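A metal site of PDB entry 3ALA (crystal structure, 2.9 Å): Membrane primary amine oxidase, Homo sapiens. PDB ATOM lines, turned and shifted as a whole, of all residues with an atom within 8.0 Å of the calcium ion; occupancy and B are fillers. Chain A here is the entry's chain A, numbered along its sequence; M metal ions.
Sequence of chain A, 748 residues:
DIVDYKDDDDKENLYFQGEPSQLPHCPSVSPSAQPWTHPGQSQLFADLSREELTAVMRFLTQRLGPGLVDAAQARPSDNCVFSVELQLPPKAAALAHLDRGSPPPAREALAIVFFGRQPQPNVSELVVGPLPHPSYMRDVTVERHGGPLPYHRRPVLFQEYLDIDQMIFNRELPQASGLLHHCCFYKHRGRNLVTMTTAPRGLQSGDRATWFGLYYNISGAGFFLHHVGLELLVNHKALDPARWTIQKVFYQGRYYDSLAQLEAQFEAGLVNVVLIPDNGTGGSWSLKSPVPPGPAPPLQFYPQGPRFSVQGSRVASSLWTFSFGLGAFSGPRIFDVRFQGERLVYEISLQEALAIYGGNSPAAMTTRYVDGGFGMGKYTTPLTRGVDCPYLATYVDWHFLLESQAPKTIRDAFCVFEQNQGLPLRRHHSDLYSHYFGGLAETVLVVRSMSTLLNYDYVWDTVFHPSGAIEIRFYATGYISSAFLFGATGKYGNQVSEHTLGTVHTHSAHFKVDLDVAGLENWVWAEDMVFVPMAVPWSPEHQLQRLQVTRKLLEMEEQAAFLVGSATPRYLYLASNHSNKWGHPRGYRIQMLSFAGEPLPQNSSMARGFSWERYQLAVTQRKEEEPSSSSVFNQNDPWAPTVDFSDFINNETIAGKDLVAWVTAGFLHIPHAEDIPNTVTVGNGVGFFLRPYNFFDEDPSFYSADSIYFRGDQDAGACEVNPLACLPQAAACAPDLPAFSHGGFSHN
ND2 of Asn 650 lies close to OE2 of Glu 652, at 3.3 Å. The backbone NH of Glu 557 lies within hydrogen-bond range of the backbone carbonyl oxygen of Glu 652. The backbone NH of Gln 621 lies close to the side-chain carboxylate of Glu 557 (3.0 Å). The side-chain carboxylate (OE1) of Glu 652 is in salt-bridge range of the side-chain amino group (NZ) of Lys 623. The side-chain amide nitrogen (NE2) of Gln 621 sits close to the side-chain carboxylate (OE1) of Glu 652, at 3.3 Å. The side-chain carboxylate (OE2) of Glu 626 is in salt-bridge range of the side-chain amino group (NZ) of Lys 623.
The calcium ion is bound by O of Phe 648 (2.2 Å). The calcium ion is bound by OD1 of Asn 650, 2.3 Å away. The calcium ion is bound by the side-chain carboxylate (OE2) of Glu 557 (2.5 Å). The calcium ion has three donor atoms within binding distance. Slightly farther from the calcium ion lies the side-chain carboxylate (OE1) of Glu 652 (2.9 Å). Slightly farther from the calcium ion lies OE1 of Glu 557 (3.0 Å).
Lys 623 touches the calcium ion (NZ to CA, 3.6 Å). Glu 626 touches the calcium ion. Six residues have an atom within 4 Å of the calcium ion: Glu 557, Lys 623, Glu 626, Phe 648, Asn 650 and Glu 652. The nearest printed residue that does not touch the calcium ion is Thr 620 (4.2 Å).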
ATOM      1  N   GLU A 557      23.992 -10.205   3.960  1.00  0.00           N
ATOM      2  CA  GLU A 557      24.517  -9.265   4.964  1.00  0.00           C
ATOM      3  C   GLU A 557      26.025  -9.201   5.006  1.00  0.00           C
ATOM      4  O   GLU A 557      26.620  -8.140   5.181  1.00  0.00           O
ATOM      5  CB  GLU A 557      24.020  -9.622   6.367  1.00  0.00           C
ATOM      6  CG  GLU A 557      22.777  -8.884   6.795  1.00  0.00           C
ATOM      7  CD  GLU A 557      22.263  -9.287   8.160  1.00  0.00           C
ATOM      8  OE1 GLU A 557      22.752 -10.255   8.777  1.00  0.00           O
ATOM      9  OE2 GLU A 557      21.333  -8.610   8.630  1.00  0.00           O
ATOM     10  N   VAL A 619      25.450  -3.006   6.506  1.00  0.00           N
ATOM     11  CA  VAL A 619      24.016  -2.990   6.272  1.00  0.00           C
ATOM     12  C   VAL A 619      23.422  -4.329   6.733  1.00  0.00           C
ATOM     13  O   VAL A 619      23.926  -5.391   6.385  1.00  0.00           O
ATOM     14  CB  VAL A 619      23.665  -2.719   4.790  1.00  0.00           C
ATOM     15  CG1 VAL A 619      22.166  -2.612   4.577  1.00  0.00           C
ATOM     16  CG2 VAL A 619      24.350  -1.485   4.345  1.00  0.00           C
ATOM     17  N   THR A 620      22.374  -4.241   7.555  1.00  0.00           N
ATOM     18  CA  THR A 620      21.698  -5.408   8.073  1.00  0.00           C
ATOM     19  C   THR A 620      20.193  -5.260   7.947  1.00  0.00           C
ATOM     20  O   THR A 620      19.686  -4.176   7.770  1.00  0.00           O
ATOM     21  CB  THR A 620      22.008  -5.590   9.521  1.00  0.00           C
ATOM     22  OG1 THR A 620      21.532  -4.461  10.226  1.00  0.00           O
ATOM     23  CG2 THR A 620      23.455  -5.702   9.731  1.00  0.00           C
ATOM     24  N   GLN A 621      19.487  -6.368   8.033  1.00  0.00           N
ATOM     25  CA  GLN A 621      18.037  -6.316   8.083  1.00  0.00           C
ATOM     26  C   GLN A 621      17.680  -5.512   9.302  1.00  0.00           C
ATOM     27  O   GLN A 621      18.302  -5.701  10.332  1.00  0.00           O
ATOM     28  CB  GLN A 621      17.437  -7.706   8.223  1.00  0.00           C
ATOM     29  CG  GLN A 621      17.410  -8.507   6.944  1.00  0.00           C
ATOM     30  CD  GLN A 621      16.673  -9.826   7.051  1.00  0.00           C
ATOM     31  OE1 GLN A 621      15.653  -9.933   7.748  1.00  0.00           O
ATOM     32  NE2 GLN A 621      17.190 -10.841   6.373  1.00  0.00           N
ATOM     33  N   ARG A 622      16.729  -4.598   9.190  1.00  0.00           N
ATOM     34  CA  ARG A 622      16.218  -3.914  10.376  1.00  0.00           C
ATOM     35  C   ARG A 622      15.266  -4.822  11.129  1.00  0.00           C
ATOM     36  O   ARG A 622      14.433  -5.481  10.508  1.00  0.00           O
ATOM     37  CB  ARG A 622      15.478  -2.650  10.024  1.00  0.00           C
ATOM     38  CG  ARG A 622      15.175  -1.827  11.245  1.00  0.00           C
ATOM     39  CD  ARG A 622      13.954  -1.010  11.068  1.00  0.00           C
ATOM     40  NE  ARG A 622      13.566  -0.264  12.276  1.00  0.00           N
ATOM     41  CZ  ARG A 622      12.930  -0.790  13.305  1.00  0.00           C
ATOM     42  NH1 ARG A 622      12.618  -2.086  13.334  1.00  0.00           N
ATOM     43  NH2 ARG A 622      12.605  -0.026  14.325  1.00  0.00           N
ATOM     44  N   LYS A 623      15.391  -4.827  12.453  1.00  0.00           N
ATOM     45  CA  LYS A 623      14.648  -5.729  13.338  1.00  0.00           C
ATOM     46  C   LYS A 623      14.337  -5.083  14.681  1.00  0.00           C
ATOM     47  O   LYS A 623      15.218  -4.497  15.295  1.00  0.00           O
ATOM     48  CB  LYS A 623      15.465  -6.990  13.580  1.00  0.00           C
ATOM     49  CG  LYS A 623      15.653  -7.878  12.365  1.00  0.00           C
ATOM     50  CD  LYS A 623      16.600  -9.029  12.682  1.00  0.00           C
ATOM     51  CE  LYS A 623      16.571 -10.105  11.627  1.00  0.00           C
ATOM     52  NZ  LYS A 623      17.780 -10.946  11.746  1.00  0.00           N
ATOM     53  N   GLU A 626      16.603  -5.643  17.496  1.00  0.00           N
ATOM     54  CA  GLU A 626      18.007  -5.168  17.311  1.00  0.00           C
ATOM     55  C   GLU A 626      18.017  -3.654  17.230  1.00  0.00           C
ATOM     56  O   GLU A 626      18.453  -3.099  16.228  1.00  0.00           O
ATOM     57  CB  GLU A 626      18.649  -5.729  16.022  1.00  0.00           C
ATOM     58  CG  GLU A 626      19.303  -7.126  16.125  1.00  0.00           C
ATOM     59  CD  GLU A 626      19.751  -7.761  14.740  1.00  0.00           C
ATOM     60  OE1 GLU A 626      20.070  -7.012  13.780  1.00  0.00           O
ATOM     61  OE2 GLU A 626      19.800  -9.018  14.604  1.00  0.00           O
ATOM     62  N   PHE A 645      27.511  -6.032  18.776  1.00  0.00           N
ATOM     63  CA  PHE A 645      27.084  -5.638  17.464  1.00  0.00           C
ATOM     64  C   PHE A 645      27.327  -6.680  16.410  1.00  0.00           C
ATOM     65  O   PHE A 645      26.485  -6.909  15.546  1.00  0.00           O
ATOM     66  CB  PHE A 645      27.794  -4.374  17.042  1.00  0.00           C
ATOM     67  CG  PHE A 645      27.448  -3.943  15.671  1.00  0.00           C
ATOM     68  CD1 PHE A 645      26.156  -3.576  15.370  1.00  0.00           C
ATOM     69  CD2 PHE A 645      28.399  -3.947  14.663  1.00  0.00           C
ATOM     70  CE1 PHE A 645      25.834  -3.205  14.119  1.00  0.00           C
ATOM     71  CE2 PHE A 645      28.076  -3.576  13.412  1.00  0.00           C
ATOM     72  CZ  PHE A 645      26.794  -3.205  13.133  1.00  0.00           C
ATOM     73  N   SER A 646      28.489  -7.307  16.448  1.00  0.00           N
ATOM     74  CA  SER A 646      28.857  -8.272  15.431  1.00  0.00           C
ATOM     75  C   SER A 646      27.790  -9.358  15.246  1.00  0.00           C
ATOM     76  O   SER A 646      27.609  -9.907  14.165  1.00  0.00           O
ATOM     77  CB  SER A 646      30.225  -8.884  15.728  1.00  0.00           C
ATOM     78  OG  SER A 646      30.150  -9.701  16.868  1.00  0.00           O
ATOM     79  N   ASP A 647      27.061  -9.672  16.312  1.00  0.00           N
ATOM     80  CA  ASP A 647      25.953 -10.632  16.220  1.00  0.00           C
ATOM     81  C   ASP A 647      24.856 -10.247  15.250  1.00  0.00           C
ATOM     82  O   ASP A 647      24.099 -11.095  14.846  1.00  0.00           O
ATOM     83  CB  ASP A 647      25.291 -10.848  17.583  1.00  0.00           C
ATOM     84  CG  ASP A 647      26.233 -11.487  18.616  1.00  0.00           C
ATOM     85  OD1 ASP A 647      27.274 -12.096  18.246  1.00  0.00           O
ATOM     86  OD2 ASP A 647      25.906 -11.379  19.815  1.00  0.00           O
ATOM     87  N   PHE A 648      24.729  -8.976  14.893  1.00  0.00           N
ATOM     88  CA  PHE A 648      23.667  -8.557  13.996  1.00  0.00           C
ATOM     89  C   PHE A 648      23.951  -9.044  12.579  1.00  0.00           C
ATOM     90  O   PHE A 648      23.036  -9.263  11.783  1.00  0.00           O
ATOM     91  CB  PHE A 648      23.552  -7.036  13.980  1.00  0.00           C
ATOM     92  CG  PHE A 648      23.116  -6.415  15.281  1.00  0.00           C
ATOM     93  CD1 PHE A 648      22.797  -5.044  15.321  1.00  0.00           C
ATOM     94  CD2 PHE A 648      23.014  -7.155  16.450  1.00  0.00           C
ATOM     95  CE1 PHE A 648      22.383  -4.443  16.488  1.00  0.00           C
ATOM     96  CE2 PHE A 648      22.607  -6.570  17.617  1.00  0.00           C
ATOM     97  CZ  PHE A 648      22.287  -5.206  17.650  1.00  0.00           C
ATOM     98  N   ILE A 649      25.225  -9.173  12.241  1.00  0.00           N
ATOM     99  CA  ILE A 649      25.654  -9.526  10.913  1.00  0.00           C
ATOM    100  C   ILE A 649      25.684 -11.015  10.897  1.00  0.00           C
ATOM    101  O   ILE A 649      26.574 -11.611  11.461  1.00  0.00           O
ATOM    102  CB  ILE A 649      27.043  -8.994  10.623  1.00  0.00           C
ATOM    103  CG1 ILE A 649      27.106  -7.470  10.758  1.00  0.00           C
ATOM    104  CG2 ILE A 649      27.501  -9.415   9.244  1.00  0.00           C
ATOM    105  CD1 ILE A 649      28.501  -6.991  11.033  1.00  0.00           C
ATOM    106  N   ASN A 650      24.697 -11.623  10.263  1.00  0.00           N
ATOM    107  CA  ASN A 650      24.388 -13.014  10.502  1.00  0.00           C
ATOM    108  C   ASN A 650      23.966 -13.792   9.268  1.00  0.00           C
ATOM    109  O   ASN A 650      23.209 -14.733   9.385  1.00  0.00           O
ATOM    110  CB  ASN A 650      23.298 -13.137  11.578  1.00  0.00           C
ATOM    111  CG  ASN A 650      21.903 -12.765  11.081  1.00  0.00           C
ATOM    112  OD1 ASN A 650      21.534 -11.587  10.964  1.00  0.00           O
ATOM    113  ND2 ASN A 650      21.109 -13.783  10.783  1.00  0.00           N
ATOM    114  N   ASN A 651      24.447 -13.418   8.085  1.00  0.00           N
ATOM    115  CA  ASN A 651      24.251 -14.278   6.922  1.00  0.00           C
ATOM    116  C   ASN A 651      22.770 -14.440   6.504  1.00  0.00           C
ATOM    117  O   ASN A 651      22.269 -15.541   6.353  1.00  0.00           O
ATOM    118  CB  ASN A 651      24.856 -15.673   7.207  1.00  0.00           C
ATOM    119  CG  ASN A 651      25.216 -16.425   5.927  1.00  0.00           C
ATOM    120  OD1 ASN A 651      25.975 -15.902   5.088  1.00  0.00           O
ATOM    121  ND2 ASN A 651      24.661 -17.652   5.762  1.00  0.00           N
ATOM    122  N   GLU A 652      22.086 -13.316   6.341  1.00  0.00           N
ATOM    123  CA  GLU A 652      20.732 -13.273   5.801  1.00  0.00           C
ATOM    124  C   GLU A 652      20.718 -12.476   4.500  1.00  0.00           C
ATOM    125  O   GLU A 652      21.708 -11.865   4.122  1.00  0.00           O
ATOM    126  CB  GLU A 652      19.788 -12.561   6.732  1.00  0.00           C
ATOM    127  CG  GLU A 652      20.058 -12.743   8.171  1.00  0.00           C
ATOM    128  CD  GLU A 652      19.220 -11.766   9.009  1.00  0.00           C
ATOM    129  OE1 GLU A 652      19.383 -10.537   8.842  1.00  0.00           O
ATOM    130  OE2 GLU A 652      18.379 -12.193   9.825  1.00  0.00           O
ATOM    131  N   THR A 653      19.559 -12.446   3.863  1.00  0.00           N
ATOM    132  CA  THR A 653      19.371 -11.621   2.710  1.00  0.00           C
ATOM    133  C   THR A 653      19.260 -10.185   3.166  1.00  0.00           C
ATOM    134  O   THR A 653      18.699  -9.897   4.217  1.00  0.00           O
ATOM    135  CB  THR A 653      18.120 -11.993   1.935  1.00  0.00           C
ATOM    136  OG1 THR A 653      18.101 -11.256   0.717  1.00  0.00           O
ATOM    137  CG2 THR A 653      16.856 -11.705   2.738  1.00  0.00           C
ATOM    138  N   ILE A 654      19.813  -9.300   2.350  1.00  0.00           N
ATOM    139  CA  ILE A 654      19.523  -7.878   2.422  1.00  0.00           C
ATOM    140  C   ILE A 654      18.974  -7.438   1.069  1.00  0.00           C
ATOM    141  O   ILE A 654      19.009  -6.272   0.745  1.00  0.00           O
ATOM    142  CB  ILE A 654      20.758  -7.086   2.840  1.00  0.00           C
ATOM    143  CG1 ILE A 654      21.986  -7.511   2.031  1.00  0.00           C
ATOM    144  CG2 ILE A 654      21.018  -7.316   4.284  1.00  0.00           C
ATOM    145  CD1 ILE A 654      23.226  -6.678   2.288  1.00  0.00           C
ATOM    146  N   VAL A 660      18.957  -1.256   7.222  1.00  0.00           N
ATOM    147  CA  VAL A 660      19.511  -0.245   8.116  1.00  0.00           C
ATOM    148  C   VAL A 660      21.017  -0.264   8.070  1.00  0.00           C
ATOM    149  O   VAL A 660      21.622  -1.310   8.280  1.00  0.00           O
ATOM    150  CB  VAL A 660      19.051  -0.446   9.575  1.00  0.00           C
ATOM    151  CG1 VAL A 660      19.346  -1.825  10.050  1.00  0.00           C
ATOM    152  CG2 VAL A 660      19.729   0.527  10.474  1.00  0.00           C
ATOM    153  N   TRP A 662      24.804   0.945   9.308  1.00  0.00           N
ATOM    154  CA  TRP A 662      25.501   1.239  10.527  1.00  0.00           C
ATOM    155  C   TRP A 662      26.900   1.763  10.202  1.00  0.00           C
ATOM    156  O   TRP A 662      27.791   1.010   9.819  1.00  0.00           O
ATOM    157  CB  TRP A 662      25.659  -0.022  11.389  1.00  0.00           C
ATOM    158  CG  TRP A 662      24.383  -0.744  11.743  1.00  0.00           C
ATOM    159  CD1 TRP A 662      23.785  -1.732  11.038  1.00  0.00           C
ATOM    160  CD2 TRP A 662      23.582  -0.559  12.920  1.00  0.00           C
ATOM    161  NE1 TRP A 662      22.647  -2.153  11.670  1.00  0.00           N
ATOM    162  CE2 TRP A 662      22.499  -1.443  12.825  1.00  0.00           C
ATOM    163  CE3 TRP A 662      23.659   0.298  14.005  1.00  0.00           C
ATOM    164  CZ2 TRP A 662      21.507  -1.502  13.801  1.00  0.00           C
ATOM    165  CZ3 TRP A 662      22.660   0.248  14.960  1.00  0.00           C
ATOM    166  CH2 TRP A 662      21.596  -0.646  14.844  1.00  0.00           C
HETATM  167 CA    CA M   1      20.948  -9.330  10.990  1.00  0.00          CA
